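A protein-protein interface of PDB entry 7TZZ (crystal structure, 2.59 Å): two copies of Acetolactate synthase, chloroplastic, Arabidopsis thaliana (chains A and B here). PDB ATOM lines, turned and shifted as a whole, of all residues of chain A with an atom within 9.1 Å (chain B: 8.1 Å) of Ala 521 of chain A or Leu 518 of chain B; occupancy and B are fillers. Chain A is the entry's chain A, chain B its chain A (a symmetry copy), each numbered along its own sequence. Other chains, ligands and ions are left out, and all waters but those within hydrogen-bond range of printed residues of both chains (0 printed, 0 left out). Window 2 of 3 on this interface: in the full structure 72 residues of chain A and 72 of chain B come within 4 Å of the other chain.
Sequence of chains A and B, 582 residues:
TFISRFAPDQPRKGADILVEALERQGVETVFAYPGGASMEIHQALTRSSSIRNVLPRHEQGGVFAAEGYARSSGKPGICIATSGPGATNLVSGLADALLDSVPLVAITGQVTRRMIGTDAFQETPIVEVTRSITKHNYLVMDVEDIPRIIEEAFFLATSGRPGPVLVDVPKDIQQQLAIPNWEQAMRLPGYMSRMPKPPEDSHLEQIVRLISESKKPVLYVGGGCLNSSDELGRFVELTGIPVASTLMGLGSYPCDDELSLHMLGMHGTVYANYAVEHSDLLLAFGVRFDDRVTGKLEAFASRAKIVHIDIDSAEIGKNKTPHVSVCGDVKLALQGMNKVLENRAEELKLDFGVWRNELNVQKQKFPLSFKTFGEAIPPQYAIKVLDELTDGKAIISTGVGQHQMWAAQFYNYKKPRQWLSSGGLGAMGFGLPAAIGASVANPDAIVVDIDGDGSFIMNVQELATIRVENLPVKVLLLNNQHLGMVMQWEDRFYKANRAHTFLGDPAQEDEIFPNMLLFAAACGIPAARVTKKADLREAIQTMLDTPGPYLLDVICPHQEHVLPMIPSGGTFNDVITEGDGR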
ATOM      1  N   PHE A 456       4.759  36.859  -2.297  1.00  0.00           N
ATOM      2  CA  PHE A 456       3.612  35.970  -2.420  1.00  0.00           C
ATOM      3  C   PHE A 456       2.721  36.029  -1.181  1.00  0.00           C
ATOM      4  O   PHE A 456       1.491  35.958  -1.288  1.00  0.00           O
ATOM      5  CB  PHE A 456       4.088  34.538  -2.669  1.00  0.00           C
ATOM      6  CG  PHE A 456       2.989  33.536  -2.687  1.00  0.00           C
ATOM      7  CD1 PHE A 456       2.182  33.411  -3.801  1.00  0.00           C
ATOM      8  CD2 PHE A 456       2.734  32.742  -1.569  1.00  0.00           C
ATOM      9  CE1 PHE A 456       1.147  32.498  -3.836  1.00  0.00           C
ATOM     10  CE2 PHE A 456       1.679  31.804  -1.579  1.00  0.00           C
ATOM     11  CZ  PHE A 456       0.881  31.690  -2.723  1.00  0.00           C
ATOM     12  N   VAL A 460      -1.697  36.710  -0.329  1.00  0.00           N
ATOM     13  CA  VAL A 460      -1.988  35.287  -0.356  1.00  0.00           C
ATOM     14  C   VAL A 460      -3.494  35.034  -0.310  1.00  0.00           C
ATOM     15  O   VAL A 460      -3.983  34.055  -0.885  1.00  0.00           O
ATOM     16  CB  VAL A 460      -1.248  34.589   0.795  1.00  0.00           C
ATOM     17  CG1 VAL A 460      -1.920  34.882   2.113  1.00  0.00           C
ATOM     18  CG2 VAL A 460      -1.206  33.115   0.550  1.00  0.00           C
ATOM     19  N   LEU A 463      -5.540  33.572  -3.271  1.00  0.00           N
ATOM     20  CA  LEU A 463      -5.678  32.159  -3.610  1.00  0.00           C
ATOM     21  C   LEU A 463      -7.139  31.726  -3.593  1.00  0.00           C
ATOM     22  O   LEU A 463      -7.571  30.949  -4.457  1.00  0.00           O
ATOM     23  CB  LEU A 463      -4.881  31.300  -2.644  1.00  0.00           C
ATOM     24  CG  LEU A 463      -3.372  31.382  -2.729  1.00  0.00           C
ATOM     25  CD1 LEU A 463      -2.786  30.506  -1.649  1.00  0.00           C
ATOM     26  CD2 LEU A 463      -2.928  30.937  -4.108  1.00  0.00           C
ATOM     27  N   ARG A 467      -9.426  30.075  -6.750  1.00  0.00           N
ATOM     28  CA  ARG A 467     -10.193  28.841  -6.632  1.00  0.00           C
ATOM     29  C   ARG A 467     -11.646  29.031  -7.054  1.00  0.00           C
ATOM     30  O   ARG A 467     -12.144  28.317  -7.929  1.00  0.00           O
ATOM     31  CB  ARG A 467     -10.135  28.314  -5.205  1.00  0.00           C
ATOM     32  CG  ARG A 467     -11.019  27.084  -5.031  1.00  0.00           C
ATOM     33  CD  ARG A 467     -10.359  25.817  -5.610  1.00  0.00           C
ATOM     34  NE  ARG A 467     -10.614  25.647  -7.036  1.00  0.00           N
ATOM     35  CZ  ARG A 467      -9.913  24.849  -7.850  1.00  0.00           C
ATOM     36  NH1 ARG A 467      -8.888  24.124  -7.380  1.00  0.00           N
ATOM     37  NH2 ARG A 467     -10.229  24.773  -9.144  1.00  0.00           N
ATOM     38  N   PRO A 514       6.787  30.138   5.919  1.00  0.00           N
ATOM     39  CA  PRO A 514       5.709  29.207   6.217  1.00  0.00           C
ATOM     40  C   PRO A 514       5.700  28.085   5.227  1.00  0.00           C
ATOM     41  O   PRO A 514       6.500  28.053   4.298  1.00  0.00           O
ATOM     42  CB  PRO A 514       4.445  30.067   6.056  1.00  0.00           C
ATOM     43  CG  PRO A 514       4.931  31.475   6.122  1.00  0.00           C
ATOM     44  CD  PRO A 514       6.265  31.447   5.505  1.00  0.00           C
ATOM     45  N   ASN A 515       4.761  27.179   5.412  1.00  0.00           N
ATOM     46  CA  ASN A 515       4.558  26.078   4.482  1.00  0.00           C
ATOM     47  C   ASN A 515       3.520  26.515   3.464  1.00  0.00           C
ATOM     48  O   ASN A 515       2.310  26.371   3.665  1.00  0.00           O
ATOM     49  CB  ASN A 515       4.127  24.844   5.246  1.00  0.00           C
ATOM     50  CG  ASN A 515       3.988  23.654   4.375  1.00  0.00           C
ATOM     51  OD1 ASN A 515       3.925  23.743   3.119  1.00  0.00           O
ATOM     52  ND2 ASN A 515       3.935  22.508   5.018  1.00  0.00           N
ATOM     53  N   MET A 516       3.998  27.057   2.351  1.00  0.00           N
ATOM     54  CA  MET A 516       3.085  27.598   1.355  1.00  0.00           C
ATOM     55  C   MET A 516       2.168  26.532   0.765  1.00  0.00           C
ATOM     56  O   MET A 516       1.106  26.870   0.227  1.00  0.00           O
ATOM     57  CB  MET A 516       3.885  28.297   0.239  1.00  0.00           C
ATOM     58  CG  MET A 516       4.819  29.464   0.709  1.00  0.00           C
ATOM     59  SD  MET A 516       3.954  30.777   1.603  1.00  0.00           S
ATOM     60  CE  MET A 516       5.174  32.106   1.570  1.00  0.00           C
ATOM     61  N   LEU A 517       2.536  25.254   0.854  1.00  0.00           N
ATOM     62  CA  LEU A 517       1.658  24.217   0.320  1.00  0.00           C
ATOM     63  C   LEU A 517       0.328  24.213   1.049  1.00  0.00           C
ATOM     64  O   LEU A 517      -0.726  24.001   0.432  1.00  0.00           O
ATOM     65  CB  LEU A 517       2.331  22.856   0.432  1.00  0.00           C
ATOM     66  CG  LEU A 517       3.747  22.847  -0.131  1.00  0.00           C
ATOM     67  CD1 LEU A 517       4.388  21.526   0.166  1.00  0.00           C
ATOM     68  CD2 LEU A 517       3.677  23.085  -1.597  1.00  0.00           C
ATOM     69  N   LEU A 518       0.359  24.474   2.368  1.00  0.00           N
ATOM     70  CA  LEU A 518      -0.864  24.504   3.167  1.00  0.00           C
ATOM     71  C   LEU A 518      -1.732  25.736   2.863  1.00  0.00           C
ATOM     72  O   LEU A 518      -2.960  25.639   2.924  1.00  0.00           O
ATOM     73  CB  LEU A 518      -0.497  24.409   4.651  1.00  0.00           C
ATOM     74  CG  LEU A 518       0.189  23.046   4.892  1.00  0.00           C
ATOM     75  CD1 LEU A 518       0.518  22.798   6.325  1.00  0.00           C
ATOM     76  CD2 LEU A 518      -0.667  21.892   4.354  1.00  0.00           C
ATOM     77  N   PHE A 519      -1.129  26.877   2.496  1.00  0.00           N
ATOM     78  CA  PHE A 519      -1.909  27.989   1.947  1.00  0.00           C
ATOM     79  C   PHE A 519      -2.693  27.547   0.727  1.00  0.00           C
ATOM     80  O   PHE A 519      -3.881  27.845   0.594  1.00  0.00           O
ATOM     81  CB  PHE A 519      -0.998  29.171   1.575  1.00  0.00           C
ATOM     82  CG  PHE A 519      -0.521  29.965   2.763  1.00  0.00           C
ATOM     83  CD1 PHE A 519      -1.419  30.554   3.622  1.00  0.00           C
ATOM     84  CD2 PHE A 519       0.825  30.113   3.023  1.00  0.00           C
ATOM     85  CE1 PHE A 519      -0.993  31.265   4.729  1.00  0.00           C
ATOM     86  CE2 PHE A 519       1.252  30.813   4.131  1.00  0.00           C
ATOM     87  CZ  PHE A 519       0.337  31.373   4.995  1.00  0.00           C
ATOM     88  N   ALA A 520      -2.029  26.856  -0.199  1.00  0.00           N
ATOM     89  CA  ALA A 520      -2.729  26.352  -1.368  1.00  0.00           C
ATOM     90  C   ALA A 520      -3.807  25.344  -0.965  1.00  0.00           C
ATOM     91  O   ALA A 520      -4.941  25.401  -1.464  1.00  0.00           O
ATOM     92  CB  ALA A 520      -1.716  25.750  -2.343  1.00  0.00           C
ATOM     93  N   ALA A 521      -3.479  24.432  -0.038  1.00  0.00           N
ATOM     94  CA  ALA A 521      -4.449  23.430   0.386  1.00  0.00           C
ATOM     95  C   ALA A 521      -5.665  24.085   1.014  1.00  0.00           C
ATOM     96  O   ALA A 521      -6.805  23.692   0.720  1.00  0.00           O
ATOM     97  CB  ALA A 521      -3.815  22.449   1.362  1.00  0.00           C
ATOM     98  N   ALA A 522      -5.439  25.094   1.877  1.00  0.00           N
ATOM     99  CA  ALA A 522      -6.549  25.853   2.463  1.00  0.00           C
ATOM    100  C   ALA A 522      -7.545  26.330   1.407  1.00  0.00           C
ATOM    101  O   ALA A 522      -8.744  26.414   1.684  1.00  0.00           O
ATOM    102  CB  ALA A 522      -6.021  27.048   3.261  1.00  0.00           C
ATOM    103  N   CYS A 523      -7.085  26.594   0.178  1.00  0.00           N
ATOM    104  CA  CYS A 523      -7.952  27.125  -0.869  1.00  0.00           C
ATOM    105  C   CYS A 523      -8.223  26.094  -1.943  1.00  0.00           C
ATOM    106  O   CYS A 523      -8.682  26.452  -3.032  1.00  0.00           O
ATOM    107  CB  CYS A 523      -7.343  28.391  -1.490  1.00  0.00           C
ATOM    108  SG  CYS A 523      -7.255  29.802  -0.305  1.00  0.00           S
ATOM    109  N   GLY A 524      -7.942  24.823  -1.657  1.00  0.00           N
ATOM    110  CA  GLY A 524      -8.263  23.763  -2.590  1.00  0.00           C
ATOM    111  C   GLY A 524      -7.465  23.831  -3.860  1.00  0.00           C
ATOM    112  O   GLY A 524      -7.964  23.476  -4.938  1.00  0.00           O
ATOM    113  N   ILE A 525      -6.236  24.310  -3.771  1.00  0.00           N
ATOM    114  CA  ILE A 525      -5.395  24.458  -4.949  1.00  0.00           C
ATOM    115  C   ILE A 525      -4.295  23.405  -4.868  1.00  0.00           C
ATOM    116  O   ILE A 525      -3.558  23.359  -3.874  1.00  0.00           O
ATOM    117  CB  ILE A 525      -4.830  25.882  -5.058  1.00  0.00           C
ATOM    118  CG1 ILE A 525      -5.973  26.858  -5.387  1.00  0.00           C
ATOM    119  CG2 ILE A 525      -3.746  25.975  -6.125  1.00  0.00           C
ATOM    120  CD1 ILE A 525      -5.559  28.343  -5.303  1.00  0.00           C
ATOM    121  N   PRO A 526      -4.202  22.511  -5.850  1.00  0.00           N
ATOM    122  CA  PRO A 526      -3.094  21.549  -5.914  1.00  0.00           C
ATOM    123  C   PRO A 526      -1.735  22.221  -5.824  1.00  0.00           C
ATOM    124  O   PRO A 526      -1.493  23.264  -6.439  1.00  0.00           O
ATOM    125  CB  PRO A 526      -3.273  20.906  -7.293  1.00  0.00           C
ATOM    126  CG  PRO A 526      -4.667  21.178  -7.670  1.00  0.00           C
ATOM    127  CD  PRO A 526      -5.084  22.435  -7.017  1.00  0.00           C
ATOM    128  N   ALA A 527      -0.818  21.558  -5.126  1.00  0.00           N
ATOM    129  CA  ALA A 527       0.483  22.147  -4.856  1.00  0.00           C
ATOM    130  C   ALA A 527       1.509  21.041  -4.648  1.00  0.00           C
ATOM    131  O   ALA A 527       1.164  19.904  -4.331  1.00  0.00           O
ATOM    132  CB  ALA A 527       0.431  23.060  -3.627  1.00  0.00           C
ATOM    133  N   ALA A 528       2.783  21.408  -4.790  1.00  0.00           N
ATOM    134  CA  ALA A 528       3.927  20.528  -4.573  1.00  0.00           C
ATOM    135  C   ALA A 528       5.141  21.392  -4.264  1.00  0.00           C
ATOM    136  O   ALA A 528       5.229  22.542  -4.711  1.00  0.00           O
ATOM    137  CB  ALA A 528       4.200  19.650  -5.803  1.00  0.00           C
ATOM    138  N   LEU A 551       0.185  25.469  -7.467  1.00  0.00           N
ATOM    139  CA  LEU A 551       1.318  26.113  -6.808  1.00  0.00           C
ATOM    140  C   LEU A 551       2.526  25.175  -6.751  1.00  0.00           C
ATOM    141  O   LEU A 551       2.434  24.061  -6.229  1.00  0.00           O
ATOM    142  CB  LEU A 551       0.949  26.547  -5.381  1.00  0.00           C
ATOM    143  CG  LEU A 551       2.183  26.881  -4.520  1.00  0.00           C
ATOM    144  CD1 LEU A 551       2.686  28.191  -4.932  1.00  0.00           C
ATOM    145  CD2 LEU A 551       1.904  26.954  -3.065  1.00  0.00           C
ATOM    146  N   VAL B 460      -4.383  37.732   6.631  1.00  0.00           N
ATOM    147  CA  VAL B 460      -4.044  36.393   7.081  1.00  0.00           C
ATOM    148  C   VAL B 460      -2.531  36.188   7.106  1.00  0.00           C
ATOM    149  O   VAL B 460      -2.012  35.445   7.945  1.00  0.00           O
ATOM    150  CB  VAL B 460      -4.756  35.358   6.197  1.00  0.00           C
ATOM    151  CG1 VAL B 460      -4.087  35.265   4.848  1.00  0.00           C
ATOM    152  CG2 VAL B 460      -4.749  34.025   6.873  1.00  0.00           C
ATOM    153  N   LEU B 463      -0.453  35.752  10.358  1.00  0.00           N
ATOM    154  CA  LEU B 463      -0.268  34.512  11.105  1.00  0.00           C
ATOM    155  C   LEU B 463       1.207  34.143  11.211  1.00  0.00           C
ATOM    156  O   LEU B 463       1.660  33.676  12.265  1.00  0.00           O
ATOM    157  CB  LEU B 463      -1.031  33.376  10.445  1.00  0.00           C
ATOM    158  CG  LEU B 463      -2.542  33.429  10.510  1.00  0.00           C
ATOM    159  CD1 LEU B 463      -3.093  32.250   9.744  1.00  0.00           C
ATOM    160  CD2 LEU B 463      -2.978  33.402  11.961  1.00  0.00           C
ATOM    161  N   PHE B 513     -15.327  27.069   3.094  1.00  0.00           N
ATOM    162  CA  PHE B 513     -14.264  27.549   2.218  1.00  0.00           C
ATOM    163  C   PHE B 513     -13.895  28.988   2.562  1.00  0.00           C
ATOM    164  O   PHE B 513     -14.784  29.850   2.687  1.00  0.00           O
ATOM    165  CB  PHE B 513     -14.662  27.466   0.735  1.00  0.00           C
ATOM    166  CG  PHE B 513     -13.559  27.867  -0.175  1.00  0.00           C
ATOM    167  CD1 PHE B 513     -12.582  26.943  -0.548  1.00  0.00           C
ATOM    168  CD2 PHE B 513     -13.446  29.197  -0.613  1.00  0.00           C
ATOM    169  CE1 PHE B 513     -11.501  27.322  -1.374  1.00  0.00           C
ATOM    170  CE2 PHE B 513     -12.395  29.589  -1.436  1.00  0.00           C
ATOM    171  CZ  PHE B 513     -11.402  28.644  -1.813  1.00  0.00           C
ATOM    172  N   PRO B 514     -12.608  29.307   2.685  1.00  0.00           N
ATOM    173  CA  PRO B 514     -11.499  28.366   2.674  1.00  0.00           C
ATOM    174  C   PRO B 514     -11.458  27.594   3.955  1.00  0.00           C
ATOM    175  O   PRO B 514     -12.260  27.815   4.855  1.00  0.00           O
ATOM    176  CB  PRO B 514     -10.265  29.277   2.564  1.00  0.00           C
ATOM    177  CG  PRO B 514     -10.798  30.582   2.081  1.00  0.00           C
ATOM    178  CD  PRO B 514     -12.133  30.696   2.684  1.00  0.00           C
ATOM    179  N   ASN B 515     -10.487  26.706   4.046  1.00  0.00           N
ATOM    180  CA  ASN B 515     -10.252  25.942   5.262  1.00  0.00           C
ATOM    181  C   ASN B 515      -9.235  26.699   6.097  1.00  0.00           C
ATOM    182  O   ASN B 515      -8.019  26.542   5.942  1.00  0.00           O
ATOM    183  CB  ASN B 515      -9.775  24.552   4.901  1.00  0.00           C
ATOM    184  CG  ASN B 515      -9.601  23.683   6.088  1.00  0.00           C
ATOM    185  OD1 ASN B 515      -9.548  24.146   7.259  1.00  0.00           O
ATOM    186  ND2 ASN B 515      -9.506  22.399   5.818  1.00  0.00           N
ATOM    187  N   MET B 516      -9.736  27.533   6.998  1.00  0.00           N
ATOM    188  CA  MET B 516      -8.847  28.379   7.782  1.00  0.00           C
ATOM    189  C   MET B 516      -7.898  27.571   8.659  1.00  0.00           C
ATOM    190  O   MET B 516      -6.850  28.090   9.066  1.00  0.00           O
ATOM    191  CB  MET B 516      -9.676  29.353   8.641  1.00  0.00           C
ATOM    192  CG  MET B 516     -10.646  30.293   7.848  1.00  0.00           C
ATOM    193  SD  MET B 516      -9.821  31.306   6.596  1.00  0.00           S
ATOM    194  CE  MET B 516     -11.086  32.541   6.235  1.00  0.00           C
ATOM    195  N   LEU B 517      -8.223  26.313   8.960  1.00  0.00           N
ATOM    196  CA  LEU B 517      -7.312  25.514   9.775  1.00  0.00           C
ATOM    197  C   LEU B 517      -5.979  25.336   9.075  1.00  0.00           C
ATOM    198  O   LEU B 517      -4.922  25.354   9.721  1.00  0.00           O
ATOM    199  CB  LEU B 517      -7.938  24.160  10.081  1.00  0.00           C
ATOM    200  CG  LEU B 517      -9.357  24.273  10.627  1.00  0.00           C
ATOM    201  CD1 LEU B 517      -9.951  22.903  10.743  1.00  0.00           C
ATOM    202  CD2 LEU B 517      -9.302  24.942  11.954  1.00  0.00           C
ATOM    203  N   LEU B 518      -6.012  25.188   7.738  1.00  0.00           N
ATOM    204  CA  LEU B 518      -4.788  25.019   6.960  1.00  0.00           C
ATOM    205  C   LEU B 518      -3.962  26.313   6.876  1.00  0.00           C
ATOM    206  O   LEU B 518      -2.732  26.244   6.841  1.00  0.00           O
ATOM    207  CB  LEU B 518      -5.143  24.471   5.575  1.00  0.00           C
ATOM    208  CG  LEU B 518      -5.781  23.076   5.758  1.00  0.00           C
ATOM    209  CD1 LEU B 518      -6.094  22.399   4.467  1.00  0.00           C
ATOM    210  CD2 LEU B 518      -4.890  22.166   6.612  1.00  0.00           C
ATOM    211  N   PHE B 519      -4.605  27.491   6.888  1.00  0.00           N
ATOM    212  CA  PHE B 519      -3.867  28.741   7.073  1.00  0.00           C
ATOM    213  C   PHE B 519      -3.074  28.713   8.366  1.00  0.00           C
ATOM    214  O   PHE B 519      -1.897  29.077   8.398  1.00  0.00           O
ATOM    215  CB  PHE B 519      -4.818  29.949   7.078  1.00  0.00           C
ATOM    216  CG  PHE B 519      -5.316  30.335   5.710  1.00  0.00           C
ATOM    217  CD1 PHE B 519      -4.434  30.669   4.709  1.00  0.00           C
ATOM    218  CD2 PHE B 519      -6.665  30.351   5.424  1.00  0.00           C
ATOM    219  CE1 PHE B 519      -4.877  31.000   3.442  1.00  0.00           C
ATOM    220  CE2 PHE B 519      -7.109  30.673   4.160  1.00  0.00           C
ATOM    221  CZ  PHE B 519      -6.209  30.980   3.163  1.00  0.00           C
ATOM    222  N   ALA B 520      -3.719  28.309   9.460  1.00  0.00           N
ATOM    223  CA  ALA B 520      -3.008  28.203  10.723  1.00  0.00           C
ATOM    224  C   ALA B 520      -1.895  27.158  10.635  1.00  0.00           C
ATOM    225  O   ALA B 520      -0.766  27.400  11.089  1.00  0.00           O
ATOM    226  CB  ALA B 520      -4.006  27.888  11.838  1.00  0.00           C
ATOM    227  N   ALA B 521      -2.187  25.999  10.027  1.00  0.00           N
ATOM    228  CA  ALA B 521      -1.182  24.950   9.917  1.00  0.00           C
ATOM    229  C   ALA B 521       0.015  25.427   9.115  1.00  0.00           C
ATOM    230  O   ALA B 521       1.165  25.179   9.507  1.00  0.00           O
ATOM    231  CB  ALA B 521      -1.777  23.700   9.284  1.00  0.00           C
ATOM    232  N   ALA B 522      -0.240  26.122   7.991  1.00  0.00           N
ATOM    233  CA  ALA B 522       0.845  26.707   7.198  1.00  0.00           C
ATOM    234  C   ALA B 522       1.820  27.512   8.057  1.00  0.00           C
ATOM    235  O   ALA B 522       3.017  27.550   7.762  1.00  0.00           O
ATOM    236  CB  ALA B 522       0.282  27.589   6.081  1.00  0.00           C
ATOM    237  N   CYS B 523       1.345  28.118   9.153  1.00  0.00           N
ATOM    238  CA  CYS B 523       2.188  28.967   9.988  1.00  0.00           C
ATOM    239  C   CYS B 523       2.488  28.315  11.321  1.00  0.00           C
ATOM    240  O   CYS B 523       2.929  28.998  12.249  1.00  0.00           O
ATOM    241  CB  CYS B 523       1.534  30.339  10.204  1.00  0.00           C
ATOM    242  SG  CYS B 523       1.404  31.326   8.650  1.00  0.00           S
ATOM    243  N   GLY B 524       2.251  27.007  11.430  1.00  0.00           N
ATOM    244  CA  GLY B 524       2.603  26.288  12.636  1.00  0.00           C
ATOM    245  C   GLY B 524       1.796  26.706  13.831  1.00  0.00           C
ATOM    246  O   GLY B 524       2.302  26.708  14.964  1.00  0.00           O
ATOM    247  N   ILE B 525       0.552  27.095  13.609  1.00  0.00           N
ATOM    248  CA  ILE B 525      -0.299  27.561  14.693  1.00  0.00           C
ATOM    249  C   ILE B 525      -1.362  26.496  14.937  1.00  0.00           C
ATOM    250  O   ILE B 525      -2.092  26.130  14.007  1.00  0.00           O
ATOM    251  CB  ILE B 525      -0.913  28.933  14.372  1.00  0.00           C
ATOM    252  CG1 ILE B 525       0.196  30.000  14.388  1.00  0.00           C
ATOM    253  CG2 ILE B 525      -2.004  29.305  15.369  1.00  0.00           C
ATOM    254  CD1 ILE B 525      -0.267  31.377  13.865  1.00  0.00           C
ATOM    255  N   ALA B 527      -4.777  24.696  15.755  1.00  0.00           N
ATOM    256  CA  ALA B 527      -6.095  25.131  15.328  1.00  0.00           C
ATOM    257  C   ALA B 527      -7.082  23.981  15.467  1.00  0.00           C
ATOM    258  O   ALA B 527      -6.697  22.814  15.503  1.00  0.00           O
ATOM    259  CB  ALA B 527      -6.068  25.635  13.881  1.00  0.00           C
ATOM    260  N   ARG B 529     -11.640  23.281  14.458  1.00  0.00           N
ATOM    261  CA  ARG B 529     -12.985  23.739  14.114  1.00  0.00           C
ATOM    262  C   ARG B 529     -14.021  23.184  15.097  1.00  0.00           C
ATOM    263  O   ARG B 529     -13.870  22.072  15.606  1.00  0.00           O
ATOM    264  CB  ARG B 529     -13.346  23.332  12.684  1.00  0.00           C
ATOM    265  CG  ARG B 529     -14.685  23.872  12.215  1.00  0.00           C
ATOM    266  CD  ARG B 529     -14.890  23.549  10.745  1.00  0.00           C
ATOM    267  NE  ARG B 529     -13.824  24.074   9.894  1.00  0.00           N
ATOM    268  CZ  ARG B 529     -13.642  23.691   8.636  1.00  0.00           C
ATOM    269  NH1 ARG B 529     -14.465  22.785   8.122  1.00  0.00           N
ATOM    270  NH2 ARG B 529     -12.654  24.196   7.897  1.00  0.00           N
ATOM    271  N   LEU B 551      -5.923  29.093  16.821  1.00  0.00           N
ATOM    272  CA  LEU B 551      -7.073  29.471  16.005  1.00  0.00           C
ATOM    273  C   LEU B 551      -8.249  28.519  16.238  1.00  0.00           C
ATOM    274  O   LEU B 551      -8.116  27.303  16.074  1.00  0.00           O
ATOM    275  CB  LEU B 551      -6.711  29.469  14.512  1.00  0.00           C
ATOM    276  CG  LEU B 551      -7.952  29.487  13.596  1.00  0.00           C
ATOM    277  CD1 LEU B 551      -8.501  30.844  13.599  1.00  0.00           C
ATOM    278  CD2 LEU B 551      -7.668  29.130  12.185  1.00  0.00           C
ATOM    279  N   ASP B 553     -11.926  27.927  14.683  1.00  0.00           N
ATOM    280  CA  ASP B 553     -12.889  28.194  13.615  1.00  0.00           C
ATOM    281  C   ASP B 553     -14.291  27.802  14.109  1.00  0.00           C
ATOM    282  O   ASP B 553     -14.618  26.620  14.177  1.00  0.00           O
ATOM    283  CB  ASP B 553     -12.466  27.404  12.376  1.00  0.00           C
ATOM    284  CG  ASP B 553     -13.214  27.810  11.093  1.00  0.00           C
ATOM    285  OD1 ASP B 553     -13.751  28.935  11.015  1.00  0.00           O
ATOM    286  OD2 ASP B 553     -13.254  26.983  10.145  1.00  0.00           O
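The backbone carbonyl oxygen (O) of Ala 522 of chain A is in hydrogen-bond range of the backbone NH (N) of Asn 515 of chain B (2.9 Å). The backbone NH (N) of Asn 515 of chain A is in hydrogen-bond range of the backbone carbonyl oxygen (O) of Ala 522 of chain B, 2.9 Å away.
The guanidinium group (NH1) of Arg 467 of chain A sits at hydrogen-bond distance from the backbone carbonyl oxygen (O) of Gly 524 of chain A (2.7 Å). The side-chain amide oxygen (OD1) of Asn 515 of chain B lies within hydrogen-bond range of the backbone NH (N) of Leu 517 of chain B (3.1 Å). NH2 of Arg 529 of chain B is in hydrogen-bond range of OD1 of Asn 515 of chain B. The side-chain amide oxygen (OD1) of Asn 515 of chain A lies within hydrogen-bond range of the backbone NH (N) of Leu 517 of chain A, at 3.1 Å.
CG1 of Val 460 of chain A touches CG1 of Val 460 of chain B, at 3.5 Å. CG of Arg 467 of chain A touches CZ of Phe 513 of chain B, at 3.6 Å. CB of Pro 514 of chain A touches O of Ala 522 of chain B, 3.4 Å away. Leu 518 of chain B touches Leu 518 of chain A. CB of Ala 522 of chain B touches CB of Leu 518 of chain A, at 3.6 Å. CD1 of Phe 519 of chain A touches CD1 of Phe 519 of chain B, at 3.2 Å. Phe 519 of chain A touches Ala 522 of chain B (CE2 to CB, 3.9 Å). Pro 514 of chain B touches Ala 522 of chain A. CB of Ala 522 of chain A touches CB of Leu 518 of chain B (3.6 Å).
Printed residues of chain B within 4 Å of Val 460 of chain A: Val 460 (3.5 Å). Printed residues of chain B within 4 Å of Pro 514 of chain A: Ala 522 (3.4 Å). Printed residues of chain B within 4 Å of Asn 515 of chain A: Ala 522 (2.9 Å). Of the printed residues of chain B, Ala 521 of chain A touches Leu 518. Ala 522 of chain A touches four residues of chain B. Of the printed residues of chain A, Pro 514 of chain B touches Ala 522 (3.4 Å). Of the printed residues of chain A, Asn 515 of chain B touches Ala 522 (2.9 Å). Printed residues of chain A within 4 Å of Leu 518 of chain B: Leu 518 (3.6 Å), Ala 521 (3.9 Å) and Ala 522 (3.6 Å). Ala 521 of chain B touches just one residue of chain A: Leu 518 (3.9 Å). The nearest residue of chain B that does not touch Ala 521 of chain A is Asn 515 of chain B (5.2 Å). The nearest residue of chain A that does not touch Leu 518 of chain B is Phe 519 of chain A (4.7 Å). The nearest printed residue of chain B that does not touch Pro 514 of chain A is Cys 523 of chain B (4.2 Å).
Hydrophobic or aromatic side chains of chain A that line the printed part of chain B: Val 460, Pro 514, Leu 518, Phe 519, Ala 521 and Ala 522. Printed residues of chain B that touch a printed residue of chain A: Val 460, Phe 513, Pro 514, Asn 515, Leu 518, Phe 519, Ala 521, Ala 522 and Cys 523. Hydrophobic or aromatic side chains of chain B that line the printed part of chain A: Val 460, Phe 513, Pro 514, Leu 518, Phe 519, Ala 521 and Ala 522. Among the printed residues, 17 pairs touch across the chains. Among the printed residues, no Asp or Glu carboxylate lies within 4 Å of a Lys or Arg side-chain nitrogen of the other chain.
Val 460 of chain A touches its own counterpart, Val 460 of chain B. Asn 515 of chain A touches Ala 522 of chain B, and with the chains exchanged Ala 522 of chain A touches Asn 515 of chain B. Leu 518 of chain A touches Ala 521 of chain B, and with the chains exchanged Ala 521 of chain A touches Leu 518 of chain B. Phe 519 of chain B touches its own counterpart, Phe 519 of chain A. Positions printed for both chains: 460, 463, 514, 515, 516, 517, 518, 519, 520, 521, 522, 523, 524, 525, 527 and 551.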
